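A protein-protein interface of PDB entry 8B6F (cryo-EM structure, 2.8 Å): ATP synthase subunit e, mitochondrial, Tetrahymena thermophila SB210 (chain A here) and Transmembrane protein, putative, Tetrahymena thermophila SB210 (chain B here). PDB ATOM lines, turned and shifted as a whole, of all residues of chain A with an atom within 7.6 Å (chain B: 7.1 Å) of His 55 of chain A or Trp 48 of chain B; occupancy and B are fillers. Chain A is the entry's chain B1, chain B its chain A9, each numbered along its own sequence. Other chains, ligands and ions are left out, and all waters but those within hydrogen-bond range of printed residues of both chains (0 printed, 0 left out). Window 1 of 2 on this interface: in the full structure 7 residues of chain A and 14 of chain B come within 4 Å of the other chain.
Of chain B, only His 26 (3.1 Å), Thr 27 (3.4 Å) and Trp 48 (3.8 Å) come within 4 Å of His 55 of chain A. Printed residues of chain A within 4 Å of His 26 of chain B: His 55 (3.1 Å). Printed residues of chain A within 4 Å of Thr 27 of chain B: His 55 (3.4 Å). Leu 28 of chain B touches none of the printed residues of chain A. Of the printed residues of chain A, Trp 48 of chain B touches His 55. The nearest printed residue of chain A that does not touch Trp 48 of chain B is Glu 48 of chain A (7.6 Å). The nearest printed residue of chain A that does not touch His 26 of chain B is Asn 56 of chain A (5.5 Å).
Of the 11 printed residues of chain A, 1 touches a printed residue of chain B. Hydrophobic or aromatic side chains of chain A that line the printed part of chain B: His 55. Among the printed residues, 3 pairs touch across the chains.
Among the printed residues, pairs that only touch across the chains: His 55 of chain A with Thr 27 of chain B (3.4 Å) and His 55 of chain A with Trp 48 of chain B (3.8 Å).
The side-chain carboxylate (OE1) of Glu 48 of chain A is in hydrogen-bond range of the backbone NH (N) of His 55 of chain A (3.2 Å). OG1 of Thr 27 of chain B sits at hydrogen-bond distance from NE2 of His 29 of chain B.
ND1 of His 26 of chain B sits at hydrogen-bond distance from NE2 of His 55 of chain A.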
ATOM      1  N   GLU A  48     -23.201  -5.124  -8.930  1.00  0.00           N
ATOM      2  CA  GLU A  48     -22.820  -5.943 -10.074  1.00  0.00           C
ATOM      3  C   GLU A  48     -24.027  -6.422 -10.871  1.00  0.00           C
ATOM      4  O   GLU A  48     -23.946  -7.444 -11.559  1.00  0.00           O
ATOM      5  CB  GLU A  48     -21.981  -7.135  -9.612  1.00  0.00           C
ATOM      6  CG  GLU A  48     -20.661  -6.737  -8.972  1.00  0.00           C
ATOM      7  CD  GLU A  48     -19.863  -7.931  -8.489  1.00  0.00           C
ATOM      8  OE1 GLU A  48     -20.403  -9.056  -8.512  1.00  0.00           O
ATOM      9  OE2 GLU A  48     -18.697  -7.743  -8.084  1.00  0.00           O
ATOM     10  N   SER A  51     -23.950  -7.421 -14.699  1.00  0.00           N
ATOM     11  CA  SER A  51     -22.561  -7.356 -15.127  1.00  0.00           C
ATOM     12  C   SER A  51     -22.230  -8.549 -16.016  1.00  0.00           C
ATOM     13  O   SER A  51     -22.650  -9.678 -15.752  1.00  0.00           O
ATOM     14  CB  SER A  51     -21.634  -7.330 -13.914  1.00  0.00           C
ATOM     15  OG  SER A  51     -20.279  -7.219 -14.311  1.00  0.00           O
ATOM     16  N   SER A  52     -21.470  -8.292 -17.082  1.00  0.00           N
ATOM     17  CA  SER A  52     -21.117  -9.362 -18.010  1.00  0.00           C
ATOM     18  C   SER A  52     -20.196 -10.389 -17.363  1.00  0.00           C
ATOM     19  O   SER A  52     -20.189 -11.556 -17.769  1.00  0.00           O
ATOM     20  CB  SER A  52     -20.460  -8.776 -19.258  1.00  0.00           C
ATOM     21  OG  SER A  52     -20.206  -9.785 -20.221  1.00  0.00           O
ATOM     22  N   HIS A  53     -19.413  -9.974 -16.370  1.00  0.00           N
ATOM     23  CA  HIS A  53     -18.518 -10.860 -15.625  1.00  0.00           C
ATOM     24  C   HIS A  53     -18.790 -10.651 -14.143  1.00  0.00           C
ATOM     25  O   HIS A  53     -18.026  -9.968 -13.449  1.00  0.00           O
ATOM     26  CB  HIS A  53     -17.051 -10.587 -15.962  1.00  0.00           C
ATOM     27  CG  HIS A  53     -16.648 -11.061 -17.323  1.00  0.00           C
ATOM     28  ND1 HIS A  53     -16.307 -12.371 -17.584  1.00  0.00           N
ATOM     29  CD2 HIS A  53     -16.526 -10.400 -18.499  1.00  0.00           C
ATOM     30  CE1 HIS A  53     -15.996 -12.497 -18.861  1.00  0.00           C
ATOM     31  NE2 HIS A  53     -16.119 -11.316 -19.439  1.00  0.00           N
ATOM     32  N   PRO A  54     -19.877 -11.223 -13.620  1.00  0.00           N
ATOM     33  CA  PRO A  54     -20.215 -11.002 -12.208  1.00  0.00           C
ATOM     34  C   PRO A  54     -19.318 -11.823 -11.293  1.00  0.00           C
ATOM     35  O   PRO A  54     -19.170 -13.035 -11.466  1.00  0.00           O
ATOM     36  CB  PRO A  54     -21.678 -11.456 -12.110  1.00  0.00           C
ATOM     37  CG  PRO A  54     -22.058 -11.977 -13.481  1.00  0.00           C
ATOM     38  CD  PRO A  54     -20.802 -12.170 -14.258  1.00  0.00           C
ATOM     39  N   HIS A  55     -18.720 -11.151 -10.316  1.00  0.00           N
ATOM     40  CA  HIS A  55     -17.865 -11.793  -9.330  1.00  0.00           C
ATOM     41  C   HIS A  55     -18.628 -12.242  -8.090  1.00  0.00           C
ATOM     42  O   HIS A  55     -18.022 -12.819  -7.181  1.00  0.00           O
ATOM     43  CB  HIS A  55     -16.745 -10.828  -8.922  1.00  0.00           C
ATOM     44  CG  HIS A  55     -15.605 -11.485  -8.211  1.00  0.00           C
ATOM     45  ND1 HIS A  55     -14.690 -12.291  -8.855  1.00  0.00           N
ATOM     46  CD2 HIS A  55     -15.227 -11.452  -6.911  1.00  0.00           C
ATOM     47  CE1 HIS A  55     -13.800 -12.727  -7.982  1.00  0.00           C
ATOM     48  NE2 HIS A  55     -14.104 -12.235  -6.795  1.00  0.00           N
ATOM     49  N   ASN A  56     -19.934 -12.002  -8.036  1.00  0.00           N
ATOM     50  CA  ASN A  56     -20.759 -12.350  -6.889  1.00  0.00           C
ATOM     51  C   ASN A  56     -21.581 -13.593  -7.206  1.00  0.00           C
ATOM     52  O   ASN A  56     -22.177 -13.690  -8.283  1.00  0.00           O
ATOM     53  CB  ASN A  56     -21.676 -11.186  -6.513  1.00  0.00           C
ATOM     54  CG  ASN A  56     -22.391 -11.410  -5.200  1.00  0.00           C
ATOM     55  OD1 ASN A  56     -22.043 -12.311  -4.438  1.00  0.00           O
ATOM     56  ND2 ASN A  56     -23.394 -10.586  -4.924  1.00  0.00           N
ATOM     57  N   HIS A  57     -21.612 -14.539  -6.265  1.00  0.00           N
ATOM     58  CA  HIS A  57     -22.307 -15.799  -6.507  1.00  0.00           C
ATOM     59  C   HIS A  57     -23.796 -15.575  -6.735  1.00  0.00           C
ATOM     60  O   HIS A  57     -24.398 -16.200  -7.615  1.00  0.00           O
ATOM     61  CB  HIS A  57     -22.084 -16.757  -5.337  1.00  0.00           C
ATOM     62  CG  HIS A  57     -22.681 -18.113  -5.545  1.00  0.00           C
ATOM     63  ND1 HIS A  57     -22.371 -18.907  -6.630  1.00  0.00           N
ATOM     64  CD2 HIS A  57     -23.566 -18.820  -4.805  1.00  0.00           C
ATOM     65  CE1 HIS A  57     -23.043 -20.041  -6.550  1.00  0.00           C
ATOM     66  NE2 HIS A  57     -23.775 -20.015  -5.451  1.00  0.00           N
ATOM     67  N   ASP A  58     -24.406 -14.676  -5.962  1.00  0.00           N
ATOM     68  CA  ASP A  58     -25.832 -14.412  -6.123  1.00  0.00           C
ATOM     69  C   ASP A  58     -26.138 -13.854  -7.506  1.00  0.00           C
ATOM     70  O   ASP A  58     -27.113 -14.262  -8.146  1.00  0.00           O
ATOM     71  CB  ASP A  58     -26.314 -13.447  -5.041  1.00  0.00           C
ATOM     72  CG  ASP A  58     -26.186 -14.026  -3.647  1.00  0.00           C
ATOM     73  OD1 ASP A  58     -26.305 -15.261  -3.504  1.00  0.00           O
ATOM     74  OD2 ASP A  58     -25.969 -13.249  -2.694  1.00  0.00           O
ATOM     75  N   GLU A  59     -25.321 -12.915  -7.983  1.00  0.00           N
ATOM     76  CA  GLU A  59     -25.542 -12.364  -9.316  1.00  0.00           C
ATOM     77  C   GLU A  59     -25.338 -13.422 -10.391  1.00  0.00           C
ATOM     78  O   GLU A  59     -26.095 -13.473 -11.367  1.00  0.00           O
ATOM     79  CB  GLU A  59     -24.614 -11.174  -9.551  1.00  0.00           C
ATOM     80  CG  GLU A  59     -24.740 -10.554 -10.936  1.00  0.00           C
ATOM     81  CD  GLU A  59     -26.147 -10.083 -11.248  1.00  0.00           C
ATOM     82  OE1 GLU A  59     -26.937  -9.893 -10.301  1.00  0.00           O
ATOM     83  OE2 GLU A  59     -26.463  -9.904 -12.441  1.00  0.00           O
ATOM     84  N   LYS A  60     -24.320 -14.272 -10.240  1.00  0.00           N
ATOM     85  CA  LYS A  60     -24.118 -15.344 -11.207  1.00  0.00           C
ATOM     86  C   LYS A  60     -25.322 -16.276 -11.245  1.00  0.00           C
ATOM     87  O   LYS A  60     -25.766 -16.686 -12.323  1.00  0.00           O
ATOM     88  CB  LYS A  60     -22.849 -16.127 -10.875  1.00  0.00           C
ATOM     89  CG  LYS A  60     -21.568 -15.346 -11.100  1.00  0.00           C
ATOM     90  CD  LYS A  60     -20.346 -16.251 -11.076  1.00  0.00           C
ATOM     91  CE  LYS A  60     -20.175 -16.932  -9.728  1.00  0.00           C
ATOM     92  NZ  LYS A  60     -18.938 -17.762  -9.679  1.00  0.00           N
ATOM     93  N   PRO B  25     -12.680 -20.113  -7.725  1.00  0.00           N
ATOM     94  CA  PRO B  25     -11.646 -19.525  -6.856  1.00  0.00           C
ATOM     95  C   PRO B  25     -12.098 -18.276  -6.122  1.00  0.00           C
ATOM     96  O   PRO B  25     -11.749 -18.098  -4.948  1.00  0.00           O
ATOM     97  CB  PRO B  25     -10.498 -19.230  -7.834  1.00  0.00           C
ATOM     98  CG  PRO B  25     -11.136 -19.179  -9.181  1.00  0.00           C
ATOM     99  CD  PRO B  25     -12.259 -20.160  -9.134  1.00  0.00           C
ATOM    100  N   HIS B  26     -12.877 -17.411  -6.769  1.00  0.00           N
ATOM    101  CA  HIS B  26     -13.327 -16.162  -6.159  1.00  0.00           C
ATOM    102  C   HIS B  26     -12.129 -15.342  -5.671  1.00  0.00           C
ATOM    103  O   HIS B  26     -11.978 -15.048  -4.485  1.00  0.00           O
ATOM    104  CB  HIS B  26     -14.309 -16.442  -5.017  1.00  0.00           C
ATOM    105  CG  HIS B  26     -14.886 -15.208  -4.399  1.00  0.00           C
ATOM    106  ND1 HIS B  26     -15.661 -14.312  -5.105  1.00  0.00           N
ATOM    107  CD2 HIS B  26     -14.805 -14.721  -3.138  1.00  0.00           C
ATOM    108  CE1 HIS B  26     -16.030 -13.327  -4.307  1.00  0.00           C
ATOM    109  NE2 HIS B  26     -15.524 -13.551  -3.107  1.00  0.00           N
ATOM    110  N   THR B  27     -11.271 -14.980  -6.623  1.00  0.00           N
ATOM    111  CA  THR B  27     -10.026 -14.285  -6.336  1.00  0.00           C
ATOM    112  C   THR B  27      -9.862 -13.108  -7.287  1.00  0.00           C
ATOM    113  O   THR B  27     -10.419 -13.088  -8.387  1.00  0.00           O
ATOM    114  CB  THR B  27      -8.820 -15.225  -6.460  1.00  0.00           C
ATOM    115  OG1 THR B  27      -8.786 -15.798  -7.772  1.00  0.00           O
ATOM    116  CG2 THR B  27      -8.901 -16.338  -5.427  1.00  0.00           C
ATOM    117  N   LEU B  28      -9.084 -12.124  -6.847  1.00  0.00           N
ATOM    118  CA  LEU B  28      -8.820 -10.915  -7.613  1.00  0.00           C
ATOM    119  C   LEU B  28      -7.399 -10.950  -8.158  1.00  0.00           C
ATOM    120  O   LEU B  28      -6.463 -11.335  -7.450  1.00  0.00           O
ATOM    121  CB  LEU B  28      -9.014  -9.669  -6.746  1.00  0.00           C
ATOM    122  CG  LEU B  28     -10.429  -9.468  -6.202  1.00  0.00           C
ATOM    123  CD1 LEU B  28     -10.448  -8.372  -5.156  1.00  0.00           C
ATOM    124  CD2 LEU B  28     -11.395  -9.147  -7.330  1.00  0.00           C
ATOM    125  N   HIS B  29      -7.241 -10.541  -9.416  1.00  0.00           N
ATOM    126  CA  HIS B  29      -5.949 -10.553 -10.102  1.00  0.00           C
ATOM    127  C   HIS B  29      -5.662  -9.158 -10.641  1.00  0.00           C
ATOM    128  O   HIS B  29      -5.879  -8.883 -11.828  1.00  0.00           O
ATOM    129  CB  HIS B  29      -5.934 -11.578 -11.236  1.00  0.00           C
ATOM    130  CG  HIS B  29      -6.072 -12.993 -10.773  1.00  0.00           C
ATOM    131  ND1 HIS B  29      -5.141 -13.605  -9.962  1.00  0.00           N
ATOM    132  CD2 HIS B  29      -7.028 -13.921 -11.012  1.00  0.00           C
ATOM    133  CE1 HIS B  29      -5.518 -14.847  -9.719  1.00  0.00           C
ATOM    134  NE2 HIS B  29      -6.660 -15.065 -10.346  1.00  0.00           N
ATOM    135  N   ALA B  42      -6.665  -4.786  -3.794  1.00  0.00           N
ATOM    136  CA  ALA B  42      -6.941  -6.123  -4.301  1.00  0.00           C
ATOM    137  C   ALA B  42      -6.485  -7.220  -3.350  1.00  0.00           C
ATOM    138  O   ALA B  42      -6.807  -8.389  -3.584  1.00  0.00           O
ATOM    139  CB  ALA B  42      -6.273  -6.312  -5.662  1.00  0.00           C
ATOM    140  N   CYS B  43      -5.741  -6.880  -2.295  1.00  0.00           N
ATOM    141  CA  CYS B  43      -5.286  -7.878  -1.336  1.00  0.00           C
ATOM    142  C   CYS B  43      -6.410  -8.421  -0.464  1.00  0.00           C
ATOM    143  O   CYS B  43      -6.180  -9.380   0.278  1.00  0.00           O
ATOM    144  CB  CYS B  43      -4.195  -7.286  -0.442  1.00  0.00           C
ATOM    145  SG  CYS B  43      -2.684  -6.830  -1.314  1.00  0.00           S
ATOM    146  N   ARG B  44      -7.607  -7.839  -0.529  1.00  0.00           N
ATOM    147  CA  ARG B  44      -8.701  -8.272   0.332  1.00  0.00           C
ATOM    148  C   ARG B  44      -9.161  -9.694   0.039  1.00  0.00           C
ATOM    149  O   ARG B  44      -9.900 -10.262   0.851  1.00  0.00           O
ATOM    150  CB  ARG B  44      -9.884  -7.311   0.198  1.00  0.00           C
ATOM    151  CG  ARG B  44     -10.548  -7.322  -1.170  1.00  0.00           C
ATOM    152  CD  ARG B  44     -11.620  -6.248  -1.269  1.00  0.00           C
ATOM    153  NE  ARG B  44     -12.412  -6.370  -2.488  1.00  0.00           N
ATOM    154  CZ  ARG B  44     -12.059  -5.879  -3.669  1.00  0.00           C
ATOM    155  NH1 ARG B  44     -10.915  -5.238  -3.839  1.00  0.00           N
ATOM    156  NH2 ARG B  44     -12.876  -6.038  -4.707  1.00  0.00           N
ATOM    157  N   ASP B  45      -8.751 -10.282  -1.086  1.00  0.00           N
ATOM    158  CA  ASP B  45      -9.169 -11.643  -1.405  1.00  0.00           C
ATOM    159  C   ASP B  45      -8.642 -12.659  -0.401  1.00  0.00           C
ATOM    160  O   ASP B  45      -9.152 -13.783  -0.352  1.00  0.00           O
ATOM    161  CB  ASP B  45      -8.714 -12.021  -2.816  1.00  0.00           C
ATOM    162  CG  ASP B  45      -7.216 -11.894  -3.002  1.00  0.00           C
ATOM    163  OD1 ASP B  45      -6.521 -11.549  -2.025  1.00  0.00           O
ATOM    164  OD2 ASP B  45      -6.734 -12.136  -4.127  1.00  0.00           O
ATOM    165  N   MET B  46      -7.636 -12.298   0.397  1.00  0.00           N
ATOM    166  CA  MET B  46      -7.197 -13.178   1.473  1.00  0.00           C
ATOM    167  C   MET B  46      -8.261 -13.325   2.550  1.00  0.00           C
ATOM    168  O   MET B  46      -8.268 -14.330   3.266  1.00  0.00           O
ATOM    169  CB  MET B  46      -5.895 -12.660   2.089  1.00  0.00           C
ATOM    170  CG  MET B  46      -6.036 -11.359   2.863  1.00  0.00           C
ATOM    171  SD  MET B  46      -4.445 -10.740   3.446  1.00  0.00           S
ATOM    172  CE  MET B  46      -4.958  -9.276   4.339  1.00  0.00           C
ATOM    173  N   LEU B  47      -9.157 -12.344   2.680  1.00  0.00           N
ATOM    174  CA  LEU B  47     -10.277 -12.456   3.602  1.00  0.00           C
ATOM    175  C   LEU B  47     -11.363 -13.385   3.080  1.00  0.00           C
ATOM    176  O   LEU B  47     -12.235 -13.795   3.854  1.00  0.00           O
ATOM    177  CB  LEU B  47     -10.871 -11.074   3.879  1.00  0.00           C
ATOM    178  CG  LEU B  47      -9.923 -10.054   4.514  1.00  0.00           C
ATOM    179  CD1 LEU B  47     -10.607  -8.705   4.647  1.00  0.00           C
ATOM    180  CD2 LEU B  47      -9.429 -10.536   5.869  1.00  0.00           C
ATOM    181  N   TRP B  48     -11.335 -13.717   1.791  1.00  0.00           N
ATOM    182  CA  TRP B  48     -12.244 -14.701   1.223  1.00  0.00           C
ATOM    183  C   TRP B  48     -11.605 -16.073   1.078  1.00  0.00           C
ATOM    184  O   TRP B  48     -12.328 -17.074   1.032  1.00  0.00           O
ATOM    185  CB  TRP B  48     -12.736 -14.235  -0.153  1.00  0.00           C
ATOM    186  CG  TRP B  48     -13.225 -12.821  -0.170  1.00  0.00           C
ATOM    187  CD1 TRP B  48     -13.760 -12.124   0.875  1.00  0.00           C
ATOM    188  CD2 TRP B  48     -13.216 -11.925  -1.287  1.00  0.00           C
ATOM    189  NE1 TRP B  48     -14.086 -10.852   0.475  1.00  0.00           N
ATOM    190  CE2 TRP B  48     -13.763 -10.704  -0.847  1.00  0.00           C
ATOM    191  CE3 TRP B  48     -12.799 -12.039  -2.617  1.00  0.00           C
ATOM    192  CZ2 TRP B  48     -13.905  -9.604  -1.690  1.00  0.00           C
ATOM    193  CZ3 TRP B  48     -12.940 -10.946  -3.453  1.00  0.00           C
ATOM    194  CH2 TRP B  48     -13.489  -9.743  -2.986  1.00  0.00           C
ATOM    195  N   ASP B  49     -10.279 -16.138   0.997  1.00  0.00           N
ATOM    196  CA  ASP B  49      -9.576 -17.411   0.908  1.00  0.00           C
ATOM    197  C   ASP B  49      -9.995 -18.332   2.044  1.00  0.00           C
ATOM    198  O   ASP B  49      -9.746 -18.041   3.217  1.00  0.00           O
ATOM    199  CB  ASP B  49      -8.066 -17.165   0.951  1.00  0.00           C
ATOM    200  CG  ASP B  49      -7.261 -18.439   0.785  1.00  0.00           C
ATOM    201  OD1 ASP B  49      -7.861 -19.492   0.484  1.00  0.00           O
ATOM    202  OD2 ASP B  49      -6.026 -18.388   0.956  1.00  0.00           O
ATOM    203  N   HIS B  50     -10.628 -19.447   1.691  1.00  0.00           N
ATOM    204  CA  HIS B  50     -11.153 -20.380   2.677  1.00  0.00           C
ATOM    205  C   HIS B  50     -10.121 -21.391   3.157  1.00  0.00           C
ATOM    206  O   HIS B  50     -10.403 -22.134   4.103  1.00  0.00           O
ATOM    207  CB  HIS B  50     -12.367 -21.124   2.103  1.00  0.00           C
ATOM    208  CG  HIS B  50     -12.058 -21.928   0.880  1.00  0.00           C
ATOM    209  ND1 HIS B  50     -12.009 -21.376  -0.383  1.00  0.00           N
ATOM    210  CD2 HIS B  50     -11.782 -23.244   0.724  1.00  0.00           C
ATOM    211  CE1 HIS B  50     -11.716 -22.317  -1.262  1.00  0.00           C
ATOM    212  NE2 HIS B  50     -11.572 -23.460  -0.616  1.00  0.00           N
ATOM    213  N   HIS B  51      -8.944 -21.442   2.539  1.00  0.00           N
ATOM    214  CA  HIS B  51      -7.881 -22.341   2.965  1.00  0.00           C
ATOM    215  C   HIS B  51      -6.971 -21.727   4.018  1.00  0.00           C
ATOM    216  O   HIS B  51      -6.057 -22.406   4.496  1.00  0.00           O
ATOM    217  CB  HIS B  51      -7.041 -22.773   1.759  1.00  0.00           C
ATOM    218  CG  HIS B  51      -7.745 -23.723   0.842  1.00  0.00           C
ATOM    219  ND1 HIS B  51      -7.399 -23.870  -0.485  1.00  0.00           N
ATOM    220  CD2 HIS B  51      -8.769 -24.580   1.060  1.00  0.00           C
ATOM    221  CE1 HIS B  51      -8.183 -24.774  -1.044  1.00  0.00           C
ATOM    222  NE2 HIS B  51      -9.024 -25.221  -0.129  1.00  0.00           N
ATOM    223  N   TRP B  52      -7.191 -20.469   4.389  1.00  0.00           N
ATOM    224  CA  TRP B  52      -6.353 -19.794   5.373  1.00  0.00           C
ATOM    225  C   TRP B  52      -6.810 -20.212   6.765  1.00  0.00           C
ATOM    226  O   TRP B  52      -7.892 -19.825   7.214  1.00  0.00           O
ATOM    227  CB  TRP B  52      -6.437 -18.282   5.186  1.00  0.00           C
ATOM    228  CG  TRP B  52      -5.361 -17.509   5.885  1.00  0.00           C
ATOM    229  CD1 TRP B  52      -4.270 -18.014   6.530  1.00  0.00           C
ATOM    230  CD2 TRP B  52      -5.276 -16.085   6.011  1.00  0.00           C
ATOM    231  NE1 TRP B  52      -3.513 -16.993   7.049  1.00  0.00           N
ATOM    232  CE2 TRP B  52      -4.111 -15.799   6.745  1.00  0.00           C
ATOM    233  CE3 TRP B  52      -6.077 -15.025   5.575  1.00  0.00           C
ATOM    234  CZ2 TRP B  52      -3.723 -14.497   7.051  1.00  0.00           C
ATOM    235  CZ3 TRP B  52      -5.692 -13.732   5.881  1.00  0.00           C
ATOM    236  CH2 TRP B  52      -4.524 -13.479   6.613  1.00  0.00           C
ATOM    237  N   ARG B  55      -7.522 -17.391   9.190  1.00  0.00           N
ATOM    238  CA  ARG B  55      -8.784 -16.743   8.857  1.00  0.00           C
ATOM    239  C   ARG B  55      -9.966 -17.567   9.349  1.00  0.00           C
ATOM    240  O   ARG B  55     -10.914 -17.032   9.934  1.00  0.00           O
ATOM    241  CB  ARG B  55      -8.875 -16.533   7.348  1.00  0.00           C
ATOM    242  CG  ARG B  55     -10.051 -15.686   6.907  1.00  0.00           C
ATOM    243  CD  ARG B  55     -10.391 -15.956   5.458  1.00  0.00           C
ATOM    244  NE  ARG B  55     -11.144 -17.194   5.298  1.00  0.00           N
ATOM    245  CZ  ARG B  55     -12.467 -17.278   5.316  1.00  0.00           C
ATOM    246  NH1 ARG B  55     -13.229 -16.210   5.481  1.00  0.00           N
ATOM    247  NH2 ARG B  55     -13.043 -18.467   5.163  1.00  0.00           N
ATOM    248  N   ASN B  56      -9.927 -18.880   9.118  1.00  0.00           N
ATOM    249  CA  ASN B  56     -11.031 -19.733   9.540  1.00  0.00           C
ATOM    250  C   ASN B  56     -11.156 -19.765  11.057  1.00  0.00           C
ATOM    251  O   ASN B  56     -12.269 -19.768  11.592  1.00  0.00           O
ATOM    252  CB  ASN B  56     -10.840 -21.145   8.991  1.00  0.00           C
ATOM    253  CG  ASN B  56     -10.791 -21.180   7.479  1.00  0.00           C
ATOM    254  OD1 ASN B  56     -11.292 -20.280   6.810  1.00  0.00           O
ATOM    255  ND2 ASN B  56     -10.190 -22.229   6.932  1.00  0.00           N
